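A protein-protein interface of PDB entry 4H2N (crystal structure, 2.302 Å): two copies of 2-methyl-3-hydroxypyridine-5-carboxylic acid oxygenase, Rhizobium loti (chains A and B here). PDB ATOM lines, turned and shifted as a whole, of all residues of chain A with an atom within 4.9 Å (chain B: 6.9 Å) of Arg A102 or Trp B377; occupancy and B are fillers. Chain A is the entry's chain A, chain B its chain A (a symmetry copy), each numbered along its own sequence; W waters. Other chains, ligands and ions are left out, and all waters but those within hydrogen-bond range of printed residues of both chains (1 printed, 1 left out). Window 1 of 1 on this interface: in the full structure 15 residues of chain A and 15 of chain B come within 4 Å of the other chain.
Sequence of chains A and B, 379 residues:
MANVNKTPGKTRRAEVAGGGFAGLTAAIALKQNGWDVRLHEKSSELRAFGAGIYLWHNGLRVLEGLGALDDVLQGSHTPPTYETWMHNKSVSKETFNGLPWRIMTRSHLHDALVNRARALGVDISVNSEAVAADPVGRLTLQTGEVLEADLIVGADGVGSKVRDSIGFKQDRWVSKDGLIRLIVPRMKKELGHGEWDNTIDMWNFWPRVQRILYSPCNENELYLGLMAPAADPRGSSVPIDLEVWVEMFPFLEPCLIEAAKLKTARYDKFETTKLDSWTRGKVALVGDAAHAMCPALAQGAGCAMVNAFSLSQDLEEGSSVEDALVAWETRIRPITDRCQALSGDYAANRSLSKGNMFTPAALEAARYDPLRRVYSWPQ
Among the printed residues, pairs that only touch across the chains: Leu A73 with Ser B376 (3.5 Å), Thr A78 with Gly B98 (3.5 Å), Gln A74 with Pro B378 (3.7 Å), Leu A73 with Pro B378 (3.7 Å), Arg A102 with Trp B377 (3.8 Å), Leu A73 with Trp B377 (3.9 Å) and Thr A78 with Asn B97 (3.99 Å).
Printed residues of chain B within 4 Å of Thr A78: Asn B97 and Gly B98.
Arg A102 touches just these residues of chain B: Asn B97 and Trp B377.
Of the printed residues of chain A, Gly B98 touches Thr A78 (3.5 Å).
Trp B377 touches two residues of chain A.
Of the printed residues of chain A, Pro B378 touches Leu A73 (3.7 Å) and Gln A74 (3.7 Å).
The nearest printed residue of chain B that does not touch Gln A74 is Gln B379 (5.5 Å).
1 position is printed for both chains.
The side-chain hydroxyl (OG1) of Thr A78 is in hydrogen-bond range of the guanidinium group (NH1) of Arg A102 (2.9 Å).
The side-chain amide nitrogen (ND2) of Asn B97 is in hydrogen-bond range of the side-chain amide oxygen (OE1) of Gln B379 (2.8 Å).
The backbone NH of Ser B376 sits at hydrogen-bond distance from the backbone carbonyl oxygen of Arg B367, at 2.8 Å.
O of Arg A102 is in hydrogen-bond range of N of Leu A55.
NH2 of Arg A102 is in hydrogen-bond range of O of Leu A73 (2.8 Å).
OG of Ser A76 is in hydrogen-bond range of NE of Arg A102, at 2.8 Å.
Hydrophobic or aromatic side chains of chain A that line the printed part of chain B: Leu A73.
Along chain A the printed residues that touch a printed residue of chain B span positions 73 to 102.
Of the 15 printed residues of chain B, 5 touch a printed residue of chain A.
Printed residues of chain B that touch a printed residue of chain A: Asn B97, Gly B98, Ser B376, Trp B377 and Pro B378.
The backbone carbonyl oxygen (O) of Asn B97 is in hydrogen-bond range of the guanidinium group (NH1) of Arg A102, 2.8 Å away.
Water W1 lies within hydrogen-bond range of the backbone NH of Gly B98 (2.7 Å) and the backbone carbonyl oxygen of Thr A78 (2.8 Å).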
ATOM      1  N   ILE A  53      24.414   3.075 -32.306  1.00  0.00           N
ATOM      2  CA  ILE A  53      23.817   4.168 -33.055  1.00  0.00           C
ATOM      3  C   ILE A  53      22.964   5.106 -32.187  1.00  0.00           C
ATOM      4  O   ILE A  53      22.261   4.666 -31.266  1.00  0.00           O
ATOM      5  CB  ILE A  53      22.981   3.627 -34.254  1.00  0.00           C
ATOM      6  CG1 ILE A  53      22.621   4.760 -35.216  1.00  0.00           C
ATOM      7  CG2 ILE A  53      21.732   2.868 -33.771  1.00  0.00           C
ATOM      8  CD1 ILE A  53      22.206   4.272 -36.578  1.00  0.00           C
ATOM      9  N   TYR A  54      23.058   6.400 -32.489  1.00  0.00           N
ATOM     10  CA  TYR A  54      22.206   7.424 -31.900  1.00  0.00           C
ATOM     11  C   TYR A  54      21.032   7.720 -32.832  1.00  0.00           C
ATOM     12  O   TYR A  54      21.229   7.932 -34.036  1.00  0.00           O
ATOM     13  CB  TYR A  54      22.978   8.734 -31.729  1.00  0.00           C
ATOM     14  CG  TYR A  54      23.992   8.797 -30.595  1.00  0.00           C
ATOM     15  CD1 TYR A  54      25.062   7.917 -30.534  1.00  0.00           C
ATOM     16  CD2 TYR A  54      23.884   9.773 -29.601  1.00  0.00           C
ATOM     17  CE1 TYR A  54      25.998   7.989 -29.490  1.00  0.00           C
ATOM     18  CE2 TYR A  54      24.810   9.858 -28.551  1.00  0.00           C
ATOM     19  CZ  TYR A  54      25.867   8.965 -28.505  1.00  0.00           C
ATOM     20  OH  TYR A  54      26.784   9.051 -27.485  1.00  0.00           O
ATOM     21  N   LEU A  55      19.818   7.745 -32.278  1.00  0.00           N
ATOM     22  CA  LEU A  55      18.663   8.288 -32.992  1.00  0.00           C
ATOM     23  C   LEU A  55      18.085   9.478 -32.255  1.00  0.00           C
ATOM     24  O   LEU A  55      18.325   9.659 -31.063  1.00  0.00           O
ATOM     25  CB  LEU A  55      17.577   7.236 -33.206  1.00  0.00           C
ATOM     26  CG  LEU A  55      17.875   6.059 -34.134  1.00  0.00           C
ATOM     27  CD1 LEU A  55      16.631   5.181 -34.253  1.00  0.00           C
ATOM     28  CD2 LEU A  55      18.343   6.554 -35.501  1.00  0.00           C
ATOM     29  N   LEU A  60      12.936   8.717 -34.272  1.00  0.00           N
ATOM     30  CA  LEU A  60      11.991   8.039 -33.402  1.00  0.00           C
ATOM     31  C   LEU A  60      10.549   8.189 -33.912  1.00  0.00           C
ATOM     32  O   LEU A  60       9.730   7.290 -33.728  1.00  0.00           O
ATOM     33  CB  LEU A  60      12.128   8.541 -31.958  1.00  0.00           C
ATOM     34  CG  LEU A  60      13.514   8.327 -31.356  1.00  0.00           C
ATOM     35  CD1 LEU A  60      13.775   9.374 -30.297  1.00  0.00           C
ATOM     36  CD2 LEU A  60      13.696   6.913 -30.805  1.00  0.00           C
ATOM     37  N   LEU A  73      12.386   1.302 -28.055  1.00  0.00           N
ATOM     38  CA  LEU A  73      12.477   1.888 -26.722  1.00  0.00           C
ATOM     39  C   LEU A  73      12.780   0.847 -25.657  1.00  0.00           C
ATOM     40  O   LEU A  73      13.595   1.084 -24.774  1.00  0.00           O
ATOM     41  CB  LEU A  73      11.197   2.641 -26.364  1.00  0.00           C
ATOM     42  CG  LEU A  73      11.013   3.922 -27.176  1.00  0.00           C
ATOM     43  CD1 LEU A  73       9.783   4.676 -26.701  1.00  0.00           C
ATOM     44  CD2 LEU A  73      12.287   4.798 -27.114  1.00  0.00           C
ATOM     45  N   GLN A  74      12.126  -0.303 -25.752  1.00  0.00           N
ATOM     46  CA  GLN A  74      12.408  -1.407 -24.848  1.00  0.00           C
ATOM     47  C   GLN A  74      13.850  -1.827 -25.050  1.00  0.00           C
ATOM     48  O   GLN A  74      14.247  -2.171 -26.168  1.00  0.00           O
ATOM     49  CB  GLN A  74      11.473  -2.589 -25.140  1.00  0.00           C
ATOM     50  CG  GLN A  74      11.549  -3.703 -24.112  1.00  0.00           C
ATOM     51  CD  GLN A  74      10.940  -3.285 -22.785  1.00  0.00           C
ATOM     52  OE1 GLN A  74       9.756  -2.928 -22.717  1.00  0.00           O
ATOM     53  NE2 GLN A  74      11.747  -3.314 -21.727  1.00  0.00           N
ATOM     54  N   SER A  76      16.613   0.069 -24.885  1.00  0.00           N
ATOM     55  CA  SER A  76      17.578   1.092 -25.294  1.00  0.00           C
ATOM     56  C   SER A  76      17.631   2.184 -24.229  1.00  0.00           C
ATOM     57  O   SER A  76      17.078   2.019 -23.156  1.00  0.00           O
ATOM     58  CB  SER A  76      17.279   1.661 -26.686  1.00  0.00           C
ATOM     59  OG  SER A  76      16.009   2.282 -26.760  1.00  0.00           O
ATOM     60  N   HIS A  77      18.274   3.305 -24.518  1.00  0.00           N
ATOM     61  CA  HIS A  77      18.677   4.198 -23.443  1.00  0.00           C
ATOM     62  C   HIS A  77      18.638   5.663 -23.863  1.00  0.00           C
ATOM     63  O   HIS A  77      19.183   6.031 -24.899  1.00  0.00           O
ATOM     64  CB  HIS A  77      20.101   3.792 -23.016  1.00  0.00           C
ATOM     65  CG  HIS A  77      20.723   4.673 -21.976  1.00  0.00           C
ATOM     66  ND1 HIS A  77      20.378   4.615 -20.643  1.00  0.00           N
ATOM     67  CD2 HIS A  77      21.712   5.596 -22.066  1.00  0.00           C
ATOM     68  CE1 HIS A  77      21.114   5.475 -19.961  1.00  0.00           C
ATOM     69  NE2 HIS A  77      21.931   6.085 -20.802  1.00  0.00           N
ATOM     70  N   THR A  78      17.980   6.506 -23.075  1.00  0.00           N
ATOM     71  CA  THR A  78      18.229   7.931 -23.186  1.00  0.00           C
ATOM     72  C   THR A  78      19.078   8.326 -21.990  1.00  0.00           C
ATOM     73  O   THR A  78      18.625   8.202 -20.854  1.00  0.00           O
ATOM     74  CB  THR A  78      16.947   8.770 -23.188  1.00  0.00           C
ATOM     75  OG1 THR A  78      16.081   8.345 -24.257  1.00  0.00           O
ATOM     76  CG2 THR A  78      17.280  10.269 -23.334  1.00  0.00           C
ATOM     77  N   PRO A 100      13.433  14.516 -27.786  1.00  0.00           N
ATOM     78  CA  PRO A 100      13.705  13.090 -27.588  1.00  0.00           C
ATOM     79  C   PRO A 100      14.925  12.581 -28.361  1.00  0.00           C
ATOM     80  O   PRO A 100      15.198  13.023 -29.477  1.00  0.00           O
ATOM     81  CB  PRO A 100      12.428  12.421 -28.098  1.00  0.00           C
ATOM     82  CG  PRO A 100      11.358  13.525 -28.002  1.00  0.00           C
ATOM     83  CD  PRO A 100      12.087  14.766 -28.345  1.00  0.00           C
ATOM     84  N   TRP A 101      15.660  11.670 -27.737  1.00  0.00           N
ATOM     85  CA  TRP A 101      16.784  10.988 -28.367  1.00  0.00           C
ATOM     86  C   TRP A 101      17.014   9.662 -27.658  1.00  0.00           C
ATOM     87  O   TRP A 101      16.378   9.377 -26.633  1.00  0.00           O
ATOM     88  CB  TRP A 101      18.056  11.845 -28.361  1.00  0.00           C
ATOM     89  CG  TRP A 101      18.556  12.284 -27.010  1.00  0.00           C
ATOM     90  CD1 TRP A 101      17.884  13.050 -26.096  1.00  0.00           C
ATOM     91  CD2 TRP A 101      19.860  12.030 -26.438  1.00  0.00           C
ATOM     92  NE1 TRP A 101      18.675  13.271 -24.990  1.00  0.00           N
ATOM     93  CE2 TRP A 101      19.889  12.659 -25.170  1.00  0.00           C
ATOM     94  CE3 TRP A 101      20.992  11.321 -26.867  1.00  0.00           C
ATOM     95  CZ2 TRP A 101      21.004  12.596 -24.323  1.00  0.00           C
ATOM     96  CZ3 TRP A 101      22.110  11.266 -26.024  1.00  0.00           C
ATOM     97  CH2 TRP A 101      22.105  11.903 -24.770  1.00  0.00           C
ATOM     98  N   ARG A 102      17.924   8.860 -28.198  1.00  0.00           N
ATOM     99  CA  ARG A 102      18.052   7.470 -27.789  1.00  0.00           C
ATOM    100  C   ARG A 102      19.330   6.827 -28.338  1.00  0.00           C
ATOM    101  O   ARG A 102      19.718   7.061 -29.479  1.00  0.00           O
ATOM    102  CB  ARG A 102      16.835   6.678 -28.275  1.00  0.00           C
ATOM    103  CG  ARG A 102      16.573   5.410 -27.496  1.00  0.00           C
ATOM    104  CD  ARG A 102      16.085   5.757 -26.092  1.00  0.00           C
ATOM    105  NE  ARG A 102      15.341   4.660 -25.498  1.00  0.00           N
ATOM    106  CZ  ARG A 102      14.689   4.727 -24.342  1.00  0.00           C
ATOM    107  NH1 ARG A 102      14.685   5.852 -23.631  1.00  0.00           N
ATOM    108  NH2 ARG A 102      14.035   3.660 -23.902  1.00  0.00           N
ATOM    109  N   ILE A 103      19.977   6.007 -27.520  1.00  0.00           N
ATOM    110  CA  ILE A 103      21.162   5.282 -27.947  1.00  0.00           C
ATOM    111  C   ILE A 103      20.858   3.798 -27.866  1.00  0.00           C
ATOM    112  O   ILE A 103      20.202   3.351 -26.921  1.00  0.00           O
ATOM    113  CB  ILE A 103      22.361   5.569 -27.032  1.00  0.00           C
ATOM    114  CG1 ILE A 103      22.616   7.070 -26.936  1.00  0.00           C
ATOM    115  CG2 ILE A 103      23.618   4.808 -27.516  1.00  0.00           C
ATOM    116  CD1 ILE A 103      23.837   7.393 -26.099  1.00  0.00           C
ATOM    117  N   MET A 104      21.370   3.036 -28.830  1.00  0.00           N
ATOM    118  CA  MET A 104      21.090   1.610 -28.904  1.00  0.00           C
ATOM    119  C   MET A 104      22.147   0.934 -29.768  1.00  0.00           C
ATOM    120  O   MET A 104      22.834   1.596 -30.539  1.00  0.00           O
ATOM    121  CB  MET A 104      19.690   1.388 -29.506  1.00  0.00           C
ATOM    122  CG  MET A 104      19.593   1.738 -31.005  1.00  0.00           C
ATOM    123  SD  MET A 104      17.958   2.322 -31.541  1.00  0.00           S
ATOM    124  CE  MET A 104      17.894   3.946 -30.773  1.00  0.00           C
ATOM    125  N   HIS B  57       4.384  12.767 -20.576  1.00  0.00           N
ATOM    126  CA  HIS B  57       4.173  12.068 -21.845  1.00  0.00           C
ATOM    127  C   HIS B  57       2.693  11.905 -22.168  1.00  0.00           C
ATOM    128  O   HIS B  57       2.253  12.292 -23.243  1.00  0.00           O
ATOM    129  CB  HIS B  57       4.879  10.703 -21.814  1.00  0.00           C
ATOM    130  CG  HIS B  57       4.451   9.759 -22.896  1.00  0.00           C
ATOM    131  ND1 HIS B  57       3.594   8.703 -22.667  1.00  0.00           N
ATOM    132  CD2 HIS B  57       4.772   9.703 -24.212  1.00  0.00           C
ATOM    133  CE1 HIS B  57       3.405   8.038 -23.792  1.00  0.00           C
ATOM    134  NE2 HIS B  57       4.105   8.625 -24.747  1.00  0.00           N
ATOM    135  N   ARG B  61       0.856  13.836 -25.238  1.00  0.00           N
ATOM    136  CA  ARG B  61       0.221  13.063 -26.313  1.00  0.00           C
ATOM    137  C   ARG B  61      -1.233  13.494 -26.542  1.00  0.00           C
ATOM    138  O   ARG B  61      -1.715  13.477 -27.680  1.00  0.00           O
ATOM    139  CB  ARG B  61       0.281  11.550 -26.035  1.00  0.00           C
ATOM    140  CG  ARG B  61       1.670  10.941 -26.145  1.00  0.00           C
ATOM    141  CD  ARG B  61       2.167  10.919 -27.604  1.00  0.00           C
ATOM    142  NE  ARG B  61       1.607   9.803 -28.371  1.00  0.00           N
ATOM    143  CZ  ARG B  61       1.939   9.501 -29.625  1.00  0.00           C
ATOM    144  NH1 ARG B  61       2.827  10.236 -30.275  1.00  0.00           N
ATOM    145  NH2 ARG B  61       1.373   8.462 -30.229  1.00  0.00           N
ATOM    146  N   PHE B  96      14.037   9.880 -15.958  1.00  0.00           N
ATOM    147  CA  PHE B  96      12.940   8.993 -16.375  1.00  0.00           C
ATOM    148  C   PHE B  96      13.215   8.270 -17.703  1.00  0.00           C
ATOM    149  O   PHE B  96      12.295   8.010 -18.487  1.00  0.00           O
ATOM    150  CB  PHE B  96      11.619   9.778 -16.455  1.00  0.00           C
ATOM    151  CG  PHE B  96      11.487  10.874 -15.413  1.00  0.00           C
ATOM    152  CD1 PHE B  96      11.447  10.564 -14.054  1.00  0.00           C
ATOM    153  CD2 PHE B  96      11.382  12.205 -15.796  1.00  0.00           C
ATOM    154  CE1 PHE B  96      11.319  11.571 -13.096  1.00  0.00           C
ATOM    155  CE2 PHE B  96      11.252  13.214 -14.855  1.00  0.00           C
ATOM    156  CZ  PHE B  96      11.219  12.897 -13.500  1.00  0.00           C
ATOM    157  N   ASN B  97      14.481   7.954 -17.943  1.00  0.00           N
ATOM    158  CA  ASN B  97      14.878   7.215 -19.136  1.00  0.00           C
ATOM    159  C   ASN B  97      14.251   7.776 -20.419  1.00  0.00           C
ATOM    160  O   ASN B  97      13.708   7.028 -21.226  1.00  0.00           O
ATOM    161  CB  ASN B  97      14.549   5.721 -18.982  1.00  0.00           C
ATOM    162  CG  ASN B  97      15.180   5.107 -17.731  1.00  0.00           C
ATOM    163  OD1 ASN B  97      16.396   4.857 -17.691  1.00  0.00           O
ATOM    164  ND2 ASN B  97      14.356   4.866 -16.699  1.00  0.00           N
ATOM    165  N   GLY B  98      14.297   9.100 -20.566  1.00  0.00           N
ATOM    166  CA  GLY B  98      13.863   9.759 -21.787  1.00  0.00           C
ATOM    167  C   GLY B  98      12.400  10.147 -21.898  1.00  0.00           C
ATOM    168  O   GLY B  98      12.034  10.875 -22.817  1.00  0.00           O
ATOM    169  N   LEU B  99      11.571   9.671 -20.970  1.00  0.00           N
ATOM    170  CA  LEU B  99      10.147   9.993 -20.950  1.00  0.00           C
ATOM    171  C   LEU B  99       9.890  11.504 -20.996  1.00  0.00           C
ATOM    172  O   LEU B  99      10.334  12.249 -20.131  1.00  0.00           O
ATOM    173  CB  LEU B  99       9.481   9.386 -19.717  1.00  0.00           C
ATOM    174  CG  LEU B  99       7.998   9.671 -19.458  1.00  0.00           C
ATOM    175  CD1 LEU B  99       7.235   8.373 -19.326  1.00  0.00           C
ATOM    176  CD2 LEU B  99       7.836  10.498 -18.188  1.00  0.00           C
ATOM    177  N   PRO B 100       9.160  11.953 -22.019  1.00  0.00           N
ATOM    178  CA  PRO B 100       8.924  13.390 -22.185  1.00  0.00           C
ATOM    179  C   PRO B 100       8.141  14.025 -21.032  1.00  0.00           C
ATOM    180  O   PRO B 100       7.249  13.404 -20.455  1.00  0.00           O
ATOM    181  CB  PRO B 100       8.119  13.459 -23.484  1.00  0.00           C
ATOM    182  CG  PRO B 100       8.462  12.145 -24.212  1.00  0.00           C
ATOM    183  CD  PRO B 100       8.591  11.152 -23.123  1.00  0.00           C
ATOM    184  N   LEU B 363       5.277   6.203 -12.382  1.00  0.00           N
ATOM    185  CA  LEU B 363       5.228   6.814 -13.709  1.00  0.00           C
ATOM    186  C   LEU B 363       4.224   6.150 -14.646  1.00  0.00           C
ATOM    187  O   LEU B 363       4.122   6.514 -15.817  1.00  0.00           O
ATOM    188  CB  LEU B 363       6.603   6.773 -14.345  1.00  0.00           C
ATOM    189  CG  LEU B 363       7.616   7.708 -13.708  1.00  0.00           C
ATOM    190  CD1 LEU B 363       8.980   7.313 -14.211  1.00  0.00           C
ATOM    191  CD2 LEU B 363       7.277   9.172 -14.030  1.00  0.00           C
ATOM    192  N   ALA B 366       2.030   8.643 -16.517  1.00  0.00           N
ATOM    193  CA  ALA B 366       2.799   9.376 -17.515  1.00  0.00           C
ATOM    194  C   ALA B 366       3.142   8.495 -18.715  1.00  0.00           C
ATOM    195  O   ALA B 366       3.172   8.983 -19.846  1.00  0.00           O
ATOM    196  CB  ALA B 366       4.057   9.966 -16.908  1.00  0.00           C
ATOM    197  N   ARG B 367       3.367   7.200 -18.466  1.00  0.00           N
ATOM    198  CA  ARG B 367       3.878   6.288 -19.505  1.00  0.00           C
ATOM    199  C   ARG B 367       2.792   5.945 -20.508  1.00  0.00           C
ATOM    200  O   ARG B 367       3.058   5.449 -21.618  1.00  0.00           O
ATOM    201  CB  ARG B 367       4.427   4.991 -18.893  1.00  0.00           C
ATOM    202  CG  ARG B 367       5.651   5.178 -18.008  1.00  0.00           C
ATOM    203  CD  ARG B 367       6.214   3.844 -17.526  1.00  0.00           C
ATOM    204  NE  ARG B 367       6.577   3.035 -18.685  1.00  0.00           N
ATOM    205  CZ  ARG B 367       6.014   1.872 -18.988  1.00  0.00           C
ATOM    206  NH1 ARG B 367       5.083   1.354 -18.182  1.00  0.00           N
ATOM    207  NH2 ARG B 367       6.393   1.230 -20.090  1.00  0.00           N
ATOM    208  N   TYR B 375       1.369   1.528 -23.305  1.00  0.00           N
ATOM    209  CA  TYR B 375       2.365   2.165 -22.455  1.00  0.00           C
ATOM    210  C   TYR B 375       3.692   2.265 -23.190  1.00  0.00           C
ATOM    211  O   TYR B 375       4.176   1.282 -23.748  1.00  0.00           O
ATOM    212  CB  TYR B 375       2.534   1.393 -21.154  1.00  0.00           C
ATOM    213  CG  TYR B 375       1.313   1.459 -20.282  1.00  0.00           C
ATOM    214  CD1 TYR B 375       0.284   0.539 -20.434  1.00  0.00           C
ATOM    215  CD2 TYR B 375       1.178   2.455 -19.315  1.00  0.00           C
ATOM    216  CE1 TYR B 375      -0.835   0.598 -19.645  1.00  0.00           C
ATOM    217  CE2 TYR B 375       0.061   2.523 -18.520  1.00  0.00           C
ATOM    218  CZ  TYR B 375      -0.945   1.586 -18.684  1.00  0.00           C
ATOM    219  OH  TYR B 375      -2.071   1.634 -17.903  1.00  0.00           O
ATOM    220  N   SER B 376       4.271   3.462 -23.179  1.00  0.00           N
ATOM    221  CA  SER B 376       5.541   3.718 -23.843  1.00  0.00           C
ATOM    222  C   SER B 376       6.637   4.046 -22.827  1.00  0.00           C
ATOM    223  O   SER B 376       6.418   3.973 -21.610  1.00  0.00           O
ATOM    224  CB  SER B 376       5.376   4.871 -24.845  1.00  0.00           C
ATOM    225  OG  SER B 376       6.492   4.987 -25.707  1.00  0.00           O
ATOM    226  N   TRP B 377       7.813   4.406 -23.339  1.00  0.00           N
ATOM    227  CA  TRP B 377       8.942   4.834 -22.509  1.00  0.00           C
ATOM    228  C   TRP B 377       9.213   3.956 -21.298  1.00  0.00           C
ATOM    229  O   TRP B 377       9.120   4.413 -20.147  1.00  0.00           O
ATOM    230  CB  TRP B 377       8.733   6.278 -22.084  1.00  0.00           C
ATOM    231  CG  TRP B 377       8.637   7.138 -23.275  1.00  0.00           C
ATOM    232  CD1 TRP B 377       7.498   7.605 -23.872  1.00  0.00           C
ATOM    233  CD2 TRP B 377       9.735   7.618 -24.059  1.00  0.00           C
ATOM    234  NE1 TRP B 377       7.827   8.361 -24.975  1.00  0.00           N
ATOM    235  CE2 TRP B 377       9.193   8.386 -25.108  1.00  0.00           C
ATOM    236  CE3 TRP B 377      11.125   7.472 -23.974  1.00  0.00           C
ATOM    237  CZ2 TRP B 377       9.994   9.008 -26.063  1.00  0.00           C
ATOM    238  CZ3 TRP B 377      11.925   8.093 -24.925  1.00  0.00           C
ATOM    239  CH2 TRP B 377      11.358   8.852 -25.955  1.00  0.00           C
ATOM    240  N   PRO B 378       9.553   2.685 -21.552  1.00  0.00           N
ATOM    241  CA  PRO B 378       9.762   1.727 -20.463  1.00  0.00           C
ATOM    242  C   PRO B 378      10.913   2.175 -19.584  1.00  0.00           C
ATOM    243  O   PRO B 378      11.842   2.837 -20.058  1.00  0.00           O
ATOM    244  CB  PRO B 378      10.099   0.427 -21.192  1.00  0.00           C
ATOM    245  CG  PRO B 378      10.650   0.878 -22.516  1.00  0.00           C
ATOM    246  CD  PRO B 378       9.899   2.121 -22.867  1.00  0.00           C
ATOM    247  N   GLN B 379      10.830   1.839 -18.305  1.00  0.00           N
ATOM    248  CA  GLN B 379      11.795   2.306 -17.327  1.00  0.00           C
ATOM    249  C   GLN B 379      12.693   1.162 -16.886  1.00  0.00           C
ATOM    250  O   GLN B 379      12.746   0.121 -17.542  1.00  0.00           O
ATOM    251  CB  GLN B 379      11.073   2.899 -16.115  1.00  0.00           C
ATOM    252  CG  GLN B 379      10.116   4.029 -16.462  1.00  0.00           C
ATOM    253  CD  GLN B 379      10.828   5.255 -17.002  1.00  0.00           C
ATOM    254  OE1 GLN B 379      11.727   5.792 -16.364  1.00  0.00           O
ATOM    255  NE2 GLN B 379      10.435   5.695 -18.189  1.00  0.00           N
ATOM    256  OXT GLN B 379      13.381   1.261 -15.864  1.00  0.00           O
HETATM  257  O   HOH W   1      16.755  10.021 -19.749  1.00  0.00           O
